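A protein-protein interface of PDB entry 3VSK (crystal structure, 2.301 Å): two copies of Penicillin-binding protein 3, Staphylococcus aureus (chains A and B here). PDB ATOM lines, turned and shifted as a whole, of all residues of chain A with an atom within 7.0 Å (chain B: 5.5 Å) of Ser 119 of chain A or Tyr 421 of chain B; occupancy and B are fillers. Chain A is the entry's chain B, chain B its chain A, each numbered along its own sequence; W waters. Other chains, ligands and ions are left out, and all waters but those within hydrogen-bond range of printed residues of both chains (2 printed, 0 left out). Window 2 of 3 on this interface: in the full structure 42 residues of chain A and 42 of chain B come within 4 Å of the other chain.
The backbone carbonyl oxygen (O) of Pro 419 of chain B is in hydrogen-bond range of the guanidinium group (NH2) of Arg 78 of chain A, at 2.5 Å. NZ of Lys 81 of chain A sits close to OH of Tyr 421 of chain B, 3.4 Å away. The side-chain carboxylate (OD1) of Asp 418 of chain B lies within salt-bridge range of the guanidinium group (NE) of Arg 78 of chain A (3.2 Å).
O of Gln 116 of chain A is in hydrogen-bond range of OG of Ser 119 of chain A, at 2.8 Å. The side-chain amino group of Lys 81 of chain A lies within salt-bridge range of the side-chain carboxylate of Glu 77 of chain A (3.5 Å). The side-chain carboxylate of Asp 82 of chain A is in salt-bridge range of the guanidinium group of Arg 78 of chain A, 3.2 Å away. NZ of Lys 81 of chain A lies close to O of Ile 121 of chain A (3.3 Å). N of Tyr 421 of chain B sits at hydrogen-bond distance from SD of Met 424 of chain B (3.6 Å). N of His 375 of chain B lies within hydrogen-bond range of OH of Tyr 420 of chain B (2.6 Å).
Among the printed residues, pairs that only touch across the chains: Lys 115 of chain A with Tyr 421 of chain B (3.5 Å), Leu 118 of chain A with Tyr 421 of chain B (3.6 Å), Arg 78 of chain A with Tyr 421 of chain B (3.6 Å), Glu 77 of chain A with Tyr 421 of chain B (3.6 Å), Lys 115 of chain A with Tyr 420 of chain B (3.7 Å) and Ser 119 of chain A with Tyr 421 of chain B (3.9 Å).
Ser 119 of chain A touches just one residue of chain B: Tyr 421. Of chain A, only Glu 77 (3.6 Å), Arg 78 (3.6 Å), Lys 81 (3.4 Å), Lys 115 (3.5 Å), Leu 118 (3.6 Å) and Ser 119 (3.9 Å) come within 4 Å of Tyr 421 of chain B. Of the printed residues of chain B, Leu 118 of chain A touches Tyr 421. Of the printed residues of chain A, Pro 419 of chain B touches Arg 78 (2.5 Å). Printed residues of chain B within 4 Å of Lys 81 of chain A: Tyr 421. Printed residues of chain B within 4 Å of Arg 78 of chain A: Asp 418 (3.2 Å), Pro 419 (2.5 Å) and Tyr 421 (3.6 Å). The nearest residue of chain B that does not touch Ser 119 of chain A is Ser 422 of chain B (4.2 Å). The nearest residue of chain A that does not touch Tyr 421 of chain B is Asp 114 of chain A (5.4 Å).
Hydrophobic or aromatic side chains of chain B that line the printed part of chain A: Pro 419 and Tyr 421. Printed residues of chain A that touch a printed residue of chain B: Glu 77, Arg 78, Lys 81, Lys 115, Leu 118 and Ser 119.
No position is printed for both chains. Of the 9 pairs that touch across the chains among the printed residues, none has its exchanged pair printed and touching as well.
Water W2 lies within hydrogen-bond range of O of Tyr 420 of chain B (2.5 Å) and NH2 of Arg 78 of chain A (3.4 Å). Water W1 lies within hydrogen-bond range of the backbone NH (N) of Ala 425 of chain B (2.6 Å), the side-chain hydroxyl (OH) of Tyr 421 of chain B (2.8 Å) and the side-chain carboxylate (OE2) of Glu 77 of chain A (2.8 Å).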
ATOM      1  N   GLU A  77       2.749 -13.702  -1.491  1.00  0.00           N
ATOM      2  CA  GLU A  77       1.592 -13.670  -2.402  1.00  0.00           C
ATOM      3  C   GLU A  77       1.216 -15.069  -2.922  1.00  0.00           C
ATOM      4  O   GLU A  77       0.031 -15.400  -3.005  1.00  0.00           O
ATOM      5  CB  GLU A  77       1.822 -12.694  -3.568  1.00  0.00           C
ATOM      6  CG  GLU A  77       1.130 -13.098  -4.851  1.00  0.00           C
ATOM      7  CD  GLU A  77       1.672 -12.353  -6.047  1.00  0.00           C
ATOM      8  OE1 GLU A  77       1.624 -11.102  -6.033  1.00  0.00           O
ATOM      9  OE2 GLU A  77       2.152 -13.009  -6.996  1.00  0.00           O
ATOM     10  N   ARG A  78       2.220 -15.884  -3.265  1.00  0.00           N
ATOM     11  CA  ARG A  78       1.963 -17.262  -3.713  1.00  0.00           C
ATOM     12  C   ARG A  78       1.259 -18.087  -2.633  1.00  0.00           C
ATOM     13  O   ARG A  78       0.293 -18.799  -2.913  1.00  0.00           O
ATOM     14  CB  ARG A  78       3.232 -17.982  -4.168  1.00  0.00           C
ATOM     15  CG  ARG A  78       2.980 -19.455  -4.408  1.00  0.00           C
ATOM     16  CD  ARG A  78       2.276 -19.670  -5.713  1.00  0.00           C
ATOM     17  NE  ARG A  78       3.221 -19.980  -6.781  1.00  0.00           N
ATOM     18  CZ  ARG A  78       3.281 -21.148  -7.413  1.00  0.00           C
ATOM     19  NH1 ARG A  78       2.443 -22.125  -7.097  1.00  0.00           N
ATOM     20  NH2 ARG A  78       4.175 -21.333  -8.372  1.00  0.00           N
ATOM     21  N   LYS A  81      -2.260 -17.267  -2.776  1.00  0.00           N
ATOM     22  CA  LYS A  81      -2.907 -17.781  -3.975  1.00  0.00           C
ATOM     23  C   LYS A  81      -3.250 -19.245  -3.757  1.00  0.00           C
ATOM     24  O   LYS A  81      -4.409 -19.625  -3.836  1.00  0.00           O
ATOM     25  CB  LYS A  81      -1.979 -17.651  -5.176  1.00  0.00           C
ATOM     26  CG  LYS A  81      -2.539 -16.876  -6.336  1.00  0.00           C
ATOM     27  CD  LYS A  81      -1.860 -15.530  -6.462  1.00  0.00           C
ATOM     28  CE  LYS A  81      -1.583 -15.205  -7.907  1.00  0.00           C
ATOM     29  NZ  LYS A  81      -1.080 -13.822  -8.088  1.00  0.00           N
ATOM     30  N   ASP A  82      -2.231 -20.054  -3.460  1.00  0.00           N
ATOM     31  CA  ASP A  82      -2.412 -21.489  -3.249  1.00  0.00           C
ATOM     32  C   ASP A  82      -3.455 -21.775  -2.199  1.00  0.00           C
ATOM     33  O   ASP A  82      -4.303 -22.642  -2.378  1.00  0.00           O
ATOM     34  CB  ASP A  82      -1.095 -22.164  -2.888  1.00  0.00           C
ATOM     35  CG  ASP A  82      -0.300 -22.548  -4.107  1.00  0.00           C
ATOM     36  OD1 ASP A  82      -0.389 -23.718  -4.526  1.00  0.00           O
ATOM     37  OD2 ASP A  82       0.395 -21.680  -4.659  1.00  0.00           O
ATOM     38  N   ASP A 111      -0.955 -29.310 -15.573  1.00  0.00           N
ATOM     39  CA  ASP A 111       0.046 -28.331 -15.137  1.00  0.00           C
ATOM     40  C   ASP A 111      -0.203 -26.963 -15.767  1.00  0.00           C
ATOM     41  O   ASP A 111       0.177 -25.944 -15.200  1.00  0.00           O
ATOM     42  CB  ASP A 111       1.473 -28.803 -15.452  1.00  0.00           C
ATOM     43  CG  ASP A 111       2.547 -27.826 -14.945  1.00  0.00           C
ATOM     44  OD1 ASP A 111       2.391 -27.277 -13.827  1.00  0.00           O
ATOM     45  OD2 ASP A 111       3.549 -27.604 -15.665  1.00  0.00           O
ATOM     46  N   TYR A 113      -3.308 -25.910 -16.443  1.00  0.00           N
ATOM     47  CA  TYR A 113      -4.506 -25.440 -15.775  1.00  0.00           C
ATOM     48  C   TYR A 113      -4.068 -24.620 -14.569  1.00  0.00           C
ATOM     49  O   TYR A 113      -4.477 -23.471 -14.394  1.00  0.00           O
ATOM     50  CB  TYR A 113      -5.351 -26.641 -15.343  1.00  0.00           C
ATOM     51  CG  TYR A 113      -6.685 -26.304 -14.727  1.00  0.00           C
ATOM     52  CD1 TYR A 113      -6.772 -25.806 -13.433  1.00  0.00           C
ATOM     53  CD2 TYR A 113      -7.854 -26.519 -15.417  1.00  0.00           C
ATOM     54  CE1 TYR A 113      -7.982 -25.513 -12.861  1.00  0.00           C
ATOM     55  CE2 TYR A 113      -9.078 -26.229 -14.848  1.00  0.00           C
ATOM     56  CZ  TYR A 113      -9.135 -25.727 -13.567  1.00  0.00           C
ATOM     57  OH  TYR A 113     -10.344 -25.428 -12.990  1.00  0.00           O
ATOM     58  N   ASP A 114      -3.206 -25.229 -13.762  1.00  0.00           N
ATOM     59  CA  ASP A 114      -2.680 -24.645 -12.536  1.00  0.00           C
ATOM     60  C   ASP A 114      -1.891 -23.365 -12.800  1.00  0.00           C
ATOM     61  O   ASP A 114      -1.988 -22.388 -12.055  1.00  0.00           O
ATOM     62  CB  ASP A 114      -1.821 -25.691 -11.837  1.00  0.00           C
ATOM     63  CG  ASP A 114      -2.571 -26.991 -11.610  1.00  0.00           C
ATOM     64  OD1 ASP A 114      -3.826 -26.963 -11.569  1.00  0.00           O
ATOM     65  OD2 ASP A 114      -1.915 -28.041 -11.469  1.00  0.00           O
ATOM     66  N   LYS A 115      -1.115 -23.382 -13.874  1.00  0.00           N
ATOM     67  CA  LYS A 115      -0.366 -22.211 -14.325  1.00  0.00           C
ATOM     68  C   LYS A 115      -1.297 -21.077 -14.771  1.00  0.00           C
ATOM     69  O   LYS A 115      -0.981 -19.902 -14.593  1.00  0.00           O
ATOM     70  CB  LYS A 115       0.592 -22.592 -15.471  1.00  0.00           C
ATOM     71  CG  LYS A 115       2.104 -22.616 -15.129  1.00  0.00           C
ATOM     72  CD  LYS A 115       2.665 -24.040 -15.041  1.00  0.00           C
ATOM     73  CE  LYS A 115       4.092 -24.127 -15.557  1.00  0.00           C
ATOM     74  NZ  LYS A 115       4.644 -25.511 -15.461  1.00  0.00           N
ATOM     75  N   GLN A 116      -2.440 -21.427 -15.356  1.00  0.00           N
ATOM     76  CA  GLN A 116      -3.390 -20.415 -15.812  1.00  0.00           C
ATOM     77  C   GLN A 116      -4.301 -19.911 -14.686  1.00  0.00           C
ATOM     78  O   GLN A 116      -4.659 -18.741 -14.650  1.00  0.00           O
ATOM     79  CB  GLN A 116      -4.202 -20.933 -16.996  1.00  0.00           C
ATOM     80  CG  GLN A 116      -3.724 -20.396 -18.345  1.00  0.00           C
ATOM     81  CD  GLN A 116      -4.187 -18.967 -18.606  1.00  0.00           C
ATOM     82  OE1 GLN A 116      -5.342 -18.728 -18.986  1.00  0.00           O
ATOM     83  NE2 GLN A 116      -3.282 -18.008 -18.409  1.00  0.00           N
ATOM     84  N   LEU A 117      -4.656 -20.792 -13.762  1.00  0.00           N
ATOM     85  CA  LEU A 117      -5.359 -20.391 -12.546  1.00  0.00           C
ATOM     86  C   LEU A 117      -4.558 -19.371 -11.733  1.00  0.00           C
ATOM     87  O   LEU A 117      -5.068 -18.319 -11.370  1.00  0.00           O
ATOM     88  CB  LEU A 117      -5.609 -21.618 -11.680  1.00  0.00           C
ATOM     89  CG  LEU A 117      -6.914 -21.757 -10.920  1.00  0.00           C
ATOM     90  CD1 LEU A 117      -6.640 -22.643  -9.736  1.00  0.00           C
ATOM     91  CD2 LEU A 117      -7.489 -20.425 -10.482  1.00  0.00           C
ATOM     92  N   LEU A 118      -3.305 -19.699 -11.437  1.00  0.00           N
ATOM     93  CA  LEU A 118      -2.452 -18.814 -10.656  1.00  0.00           C
ATOM     94  C   LEU A 118      -2.395 -17.409 -11.271  1.00  0.00           C
ATOM     95  O   LEU A 118      -2.433 -16.424 -10.545  1.00  0.00           O
ATOM     96  CB  LEU A 118      -1.037 -19.415 -10.466  1.00  0.00           C
ATOM     97  CG  LEU A 118      -0.670 -20.156  -9.164  1.00  0.00           C
ATOM     98  CD1 LEU A 118      -1.871 -20.764  -8.486  1.00  0.00           C
ATOM     99  CD2 LEU A 118       0.373 -21.231  -9.438  1.00  0.00           C
ATOM    100  N   SER A 119      -2.333 -17.310 -12.599  1.00  0.00           N
ATOM    101  CA  SER A 119      -2.246 -15.998 -13.249  1.00  0.00           C
ATOM    102  C   SER A 119      -3.533 -15.176 -13.124  1.00  0.00           C
ATOM    103  O   SER A 119      -3.484 -13.945 -13.082  1.00  0.00           O
ATOM    104  CB  SER A 119      -1.812 -16.116 -14.716  1.00  0.00           C
ATOM    105  OG  SER A 119      -2.792 -16.777 -15.490  1.00  0.00           O
ATOM    106  N   LYS A 120      -4.673 -15.865 -13.039  1.00  0.00           N
ATOM    107  CA  LYS A 120      -5.997 -15.225 -12.989  1.00  0.00           C
ATOM    108  C   LYS A 120      -6.388 -14.760 -11.595  1.00  0.00           C
ATOM    109  O   LYS A 120      -7.204 -13.848 -11.446  1.00  0.00           O
ATOM    110  CB  LYS A 120      -7.081 -16.175 -13.494  1.00  0.00           C
ATOM    111  CG  LYS A 120      -7.233 -16.200 -14.979  1.00  0.00           C
ATOM    112  CD  LYS A 120      -7.862 -17.502 -15.404  1.00  0.00           C
ATOM    113  CE  LYS A 120      -8.277 -17.436 -16.855  1.00  0.00           C
ATOM    114  NZ  LYS A 120      -9.264 -18.492 -17.202  1.00  0.00           N
ATOM    115  N   ILE A 121      -5.837 -15.411 -10.578  1.00  0.00           N
ATOM    116  CA  ILE A 121      -6.133 -15.037  -9.206  1.00  0.00           C
ATOM    117  C   ILE A 121      -5.465 -13.700  -8.921  1.00  0.00           C
ATOM    118  O   ILE A 121      -4.241 -13.624  -8.865  1.00  0.00           O
ATOM    119  CB  ILE A 121      -5.610 -16.090  -8.203  1.00  0.00           C
ATOM    120  CG1 ILE A 121      -6.326 -17.430  -8.397  1.00  0.00           C
ATOM    121  CG2 ILE A 121      -5.801 -15.596  -6.797  1.00  0.00           C
ATOM    122  CD1 ILE A 121      -5.465 -18.633  -8.099  1.00  0.00           C
ATOM    123  N   ARG A 122      -6.252 -12.643  -8.743  1.00  0.00           N
ATOM    124  CA  ARG A 122      -5.663 -11.328  -8.497  1.00  0.00           C
ATOM    125  C   ARG A 122      -5.604 -10.927  -7.022  1.00  0.00           C
ATOM    126  O   ARG A 122      -6.094 -11.636  -6.141  1.00  0.00           O
ATOM    127  CB  ARG A 122      -6.336 -10.247  -9.338  1.00  0.00           C
ATOM    128  CG  ARG A 122      -5.758 -10.143 -10.740  1.00  0.00           C
ATOM    129  CD  ARG A 122      -4.266  -9.875 -10.661  1.00  0.00           C
ATOM    130  NE  ARG A 122      -4.018  -8.620  -9.958  1.00  0.00           N
ATOM    131  CZ  ARG A 122      -3.329  -7.606 -10.466  1.00  0.00           C
ATOM    132  NH1 ARG A 122      -3.164  -6.495  -9.760  1.00  0.00           N
ATOM    133  NH2 ARG A 122      -2.787  -7.716 -11.670  1.00  0.00           N
ATOM    134  N   LYS A 123      -4.992  -9.778  -6.775  1.00  0.00           N
ATOM    135  CA  LYS A 123      -4.733  -9.314  -5.430  1.00  0.00           C
ATOM    136  C   LYS A 123      -6.017  -8.944  -4.691  1.00  0.00           C
ATOM    137  O   LYS A 123      -6.069  -9.060  -3.471  1.00  0.00           O
ATOM    138  CB  LYS A 123      -3.748  -8.140  -5.473  1.00  0.00           C
ATOM    139  CG  LYS A 123      -3.105  -7.923  -6.853  1.00  0.00           C
ATOM    140  CD  LYS A 123      -1.582  -8.077  -6.824  1.00  0.00           C
ATOM    141  CE  LYS A 123      -0.973  -8.101  -8.228  1.00  0.00           C
ATOM    142  NZ  LYS A 123      -1.382  -9.296  -9.017  1.00  0.00           N
ATOM    143  N   HIS B 375       8.556 -15.611 -18.589  1.00  0.00           N
ATOM    144  CA  HIS B 375       7.872 -14.320 -18.590  1.00  0.00           C
ATOM    145  C   HIS B 375       7.411 -13.869 -17.211  1.00  0.00           C
ATOM    146  O   HIS B 375       6.761 -14.613 -16.481  1.00  0.00           O
ATOM    147  CB  HIS B 375       6.724 -14.313 -19.620  1.00  0.00           C
ATOM    148  CG  HIS B 375       7.105 -14.945 -20.926  1.00  0.00           C
ATOM    149  ND1 HIS B 375       6.869 -16.272 -21.202  1.00  0.00           N
ATOM    150  CD2 HIS B 375       7.740 -14.436 -22.010  1.00  0.00           C
ATOM    151  CE1 HIS B 375       7.330 -16.554 -22.411  1.00  0.00           C
ATOM    152  NE2 HIS B 375       7.861 -15.459 -22.921  1.00  0.00           N
ATOM    153  N   ASP B 418       8.123 -20.615  -4.598  1.00  0.00           N
ATOM    154  CA  ASP B 418       7.329 -19.872  -5.580  1.00  0.00           C
ATOM    155  C   ASP B 418       7.633 -20.342  -7.013  1.00  0.00           C
ATOM    156  O   ASP B 418       8.155 -19.567  -7.818  1.00  0.00           O
ATOM    157  CB  ASP B 418       7.661 -18.375  -5.409  1.00  0.00           C
ATOM    158  CG  ASP B 418       6.769 -17.452  -6.219  1.00  0.00           C
ATOM    159  OD1 ASP B 418       5.636 -17.834  -6.642  1.00  0.00           O
ATOM    160  OD2 ASP B 418       7.220 -16.300  -6.414  1.00  0.00           O
ATOM    161  N   PRO B 419       7.313 -21.617  -7.334  1.00  0.00           N
ATOM    162  CA  PRO B 419       7.643 -22.205  -8.643  1.00  0.00           C
ATOM    163  C   PRO B 419       7.135 -21.347  -9.786  1.00  0.00           C
ATOM    164  O   PRO B 419       6.191 -20.586  -9.595  1.00  0.00           O
ATOM    165  CB  PRO B 419       6.877 -23.533  -8.638  1.00  0.00           C
ATOM    166  CG  PRO B 419       6.760 -23.890  -7.198  1.00  0.00           C
ATOM    167  CD  PRO B 419       6.619 -22.583  -6.461  1.00  0.00           C
ATOM    168  N   TYR B 420       7.748 -21.475 -10.957  1.00  0.00           N
ATOM    169  CA  TYR B 420       7.371 -20.671 -12.103  1.00  0.00           C
ATOM    170  C   TYR B 420       5.977 -20.990 -12.621  1.00  0.00           C
ATOM    171  O   TYR B 420       5.646 -22.144 -12.888  1.00  0.00           O
ATOM    172  CB  TYR B 420       8.367 -20.868 -13.249  1.00  0.00           C
ATOM    173  CG  TYR B 420       8.058 -20.040 -14.482  1.00  0.00           C
ATOM    174  CD1 TYR B 420       8.487 -18.723 -14.568  1.00  0.00           C
ATOM    175  CD2 TYR B 420       7.354 -20.576 -15.566  1.00  0.00           C
ATOM    176  CE1 TYR B 420       8.227 -17.956 -15.693  1.00  0.00           C
ATOM    177  CE2 TYR B 420       7.083 -19.805 -16.704  1.00  0.00           C
ATOM    178  CZ  TYR B 420       7.524 -18.493 -16.758  1.00  0.00           C
ATOM    179  OH  TYR B 420       7.276 -17.701 -17.865  1.00  0.00           O
ATOM    180  N   TYR B 421       5.163 -19.943 -12.735  1.00  0.00           N
ATOM    181  CA  TYR B 421       4.040 -19.905 -13.662  1.00  0.00           C
ATOM    182  C   TYR B 421       4.213 -18.669 -14.549  1.00  0.00           C
ATOM    183  O   TYR B 421       4.644 -17.621 -14.069  1.00  0.00           O
ATOM    184  CB  TYR B 421       2.688 -19.927 -12.952  1.00  0.00           C
ATOM    185  CG  TYR B 421       2.403 -18.824 -11.955  1.00  0.00           C
ATOM    186  CD1 TYR B 421       1.665 -17.703 -12.320  1.00  0.00           C
ATOM    187  CD2 TYR B 421       2.812 -18.933 -10.628  1.00  0.00           C
ATOM    188  CE1 TYR B 421       1.364 -16.704 -11.405  1.00  0.00           C
ATOM    189  CE2 TYR B 421       2.516 -17.934  -9.691  1.00  0.00           C
ATOM    190  CZ  TYR B 421       1.792 -16.822 -10.093  1.00  0.00           C
ATOM    191  OH  TYR B 421       1.500 -15.827  -9.189  1.00  0.00           O
ATOM    192  N   SER B 422       3.922 -18.793 -15.843  1.00  0.00           N
ATOM    193  CA  SER B 422       4.125 -17.670 -16.755  1.00  0.00           C
ATOM    194  C   SER B 422       3.346 -16.427 -16.331  1.00  0.00           C
ATOM    195  O   SER B 422       2.157 -16.496 -16.018  1.00  0.00           O
ATOM    196  CB  SER B 422       3.778 -18.041 -18.198  1.00  0.00           C
ATOM    197  OG  SER B 422       3.880 -16.895 -19.027  1.00  0.00           O
ATOM    198  N   GLY B 423       4.030 -15.289 -16.315  1.00  0.00           N
ATOM    199  CA  GLY B 423       3.424 -14.041 -15.890  1.00  0.00           C
ATOM    200  C   GLY B 423       3.158 -13.974 -14.397  1.00  0.00           C
ATOM    201  O   GLY B 423       2.125 -13.459 -13.958  1.00  0.00           O
ATOM    202  N   MET B 424       4.088 -14.508 -13.615  1.00  0.00           N
ATOM    203  CA  MET B 424       4.024 -14.398 -12.167  1.00  0.00           C
ATOM    204  C   MET B 424       4.742 -13.112 -11.797  1.00  0.00           C
ATOM    205  O   MET B 424       5.559 -12.635 -12.565  1.00  0.00           O
ATOM    206  CB  MET B 424       4.737 -15.597 -11.529  1.00  0.00           C
ATOM    207  CG  MET B 424       6.237 -15.631 -11.820  1.00  0.00           C
ATOM    208  SD  MET B 424       7.046 -17.198 -11.420  1.00  0.00           S
ATOM    209  CE  MET B 424       6.676 -17.290  -9.656  1.00  0.00           C
ATOM    210  N   ALA B 425       4.437 -12.516 -10.656  1.00  0.00           N
ATOM    211  CA  ALA B 425       5.332 -11.477 -10.183  1.00  0.00           C
ATOM    212  C   ALA B 425       6.542 -12.205  -9.587  1.00  0.00           C
ATOM    213  O   ALA B 425       6.382 -13.252  -8.942  1.00  0.00           O
ATOM    214  CB  ALA B 425       4.669 -10.576  -9.159  1.00  0.00           C
HETATM  215  O   HOH W   1       2.064 -13.198  -9.799  1.00  0.00           O
HETATM  216  O   HOH W   2       4.390 -23.336 -11.049  1.00  0.00           O
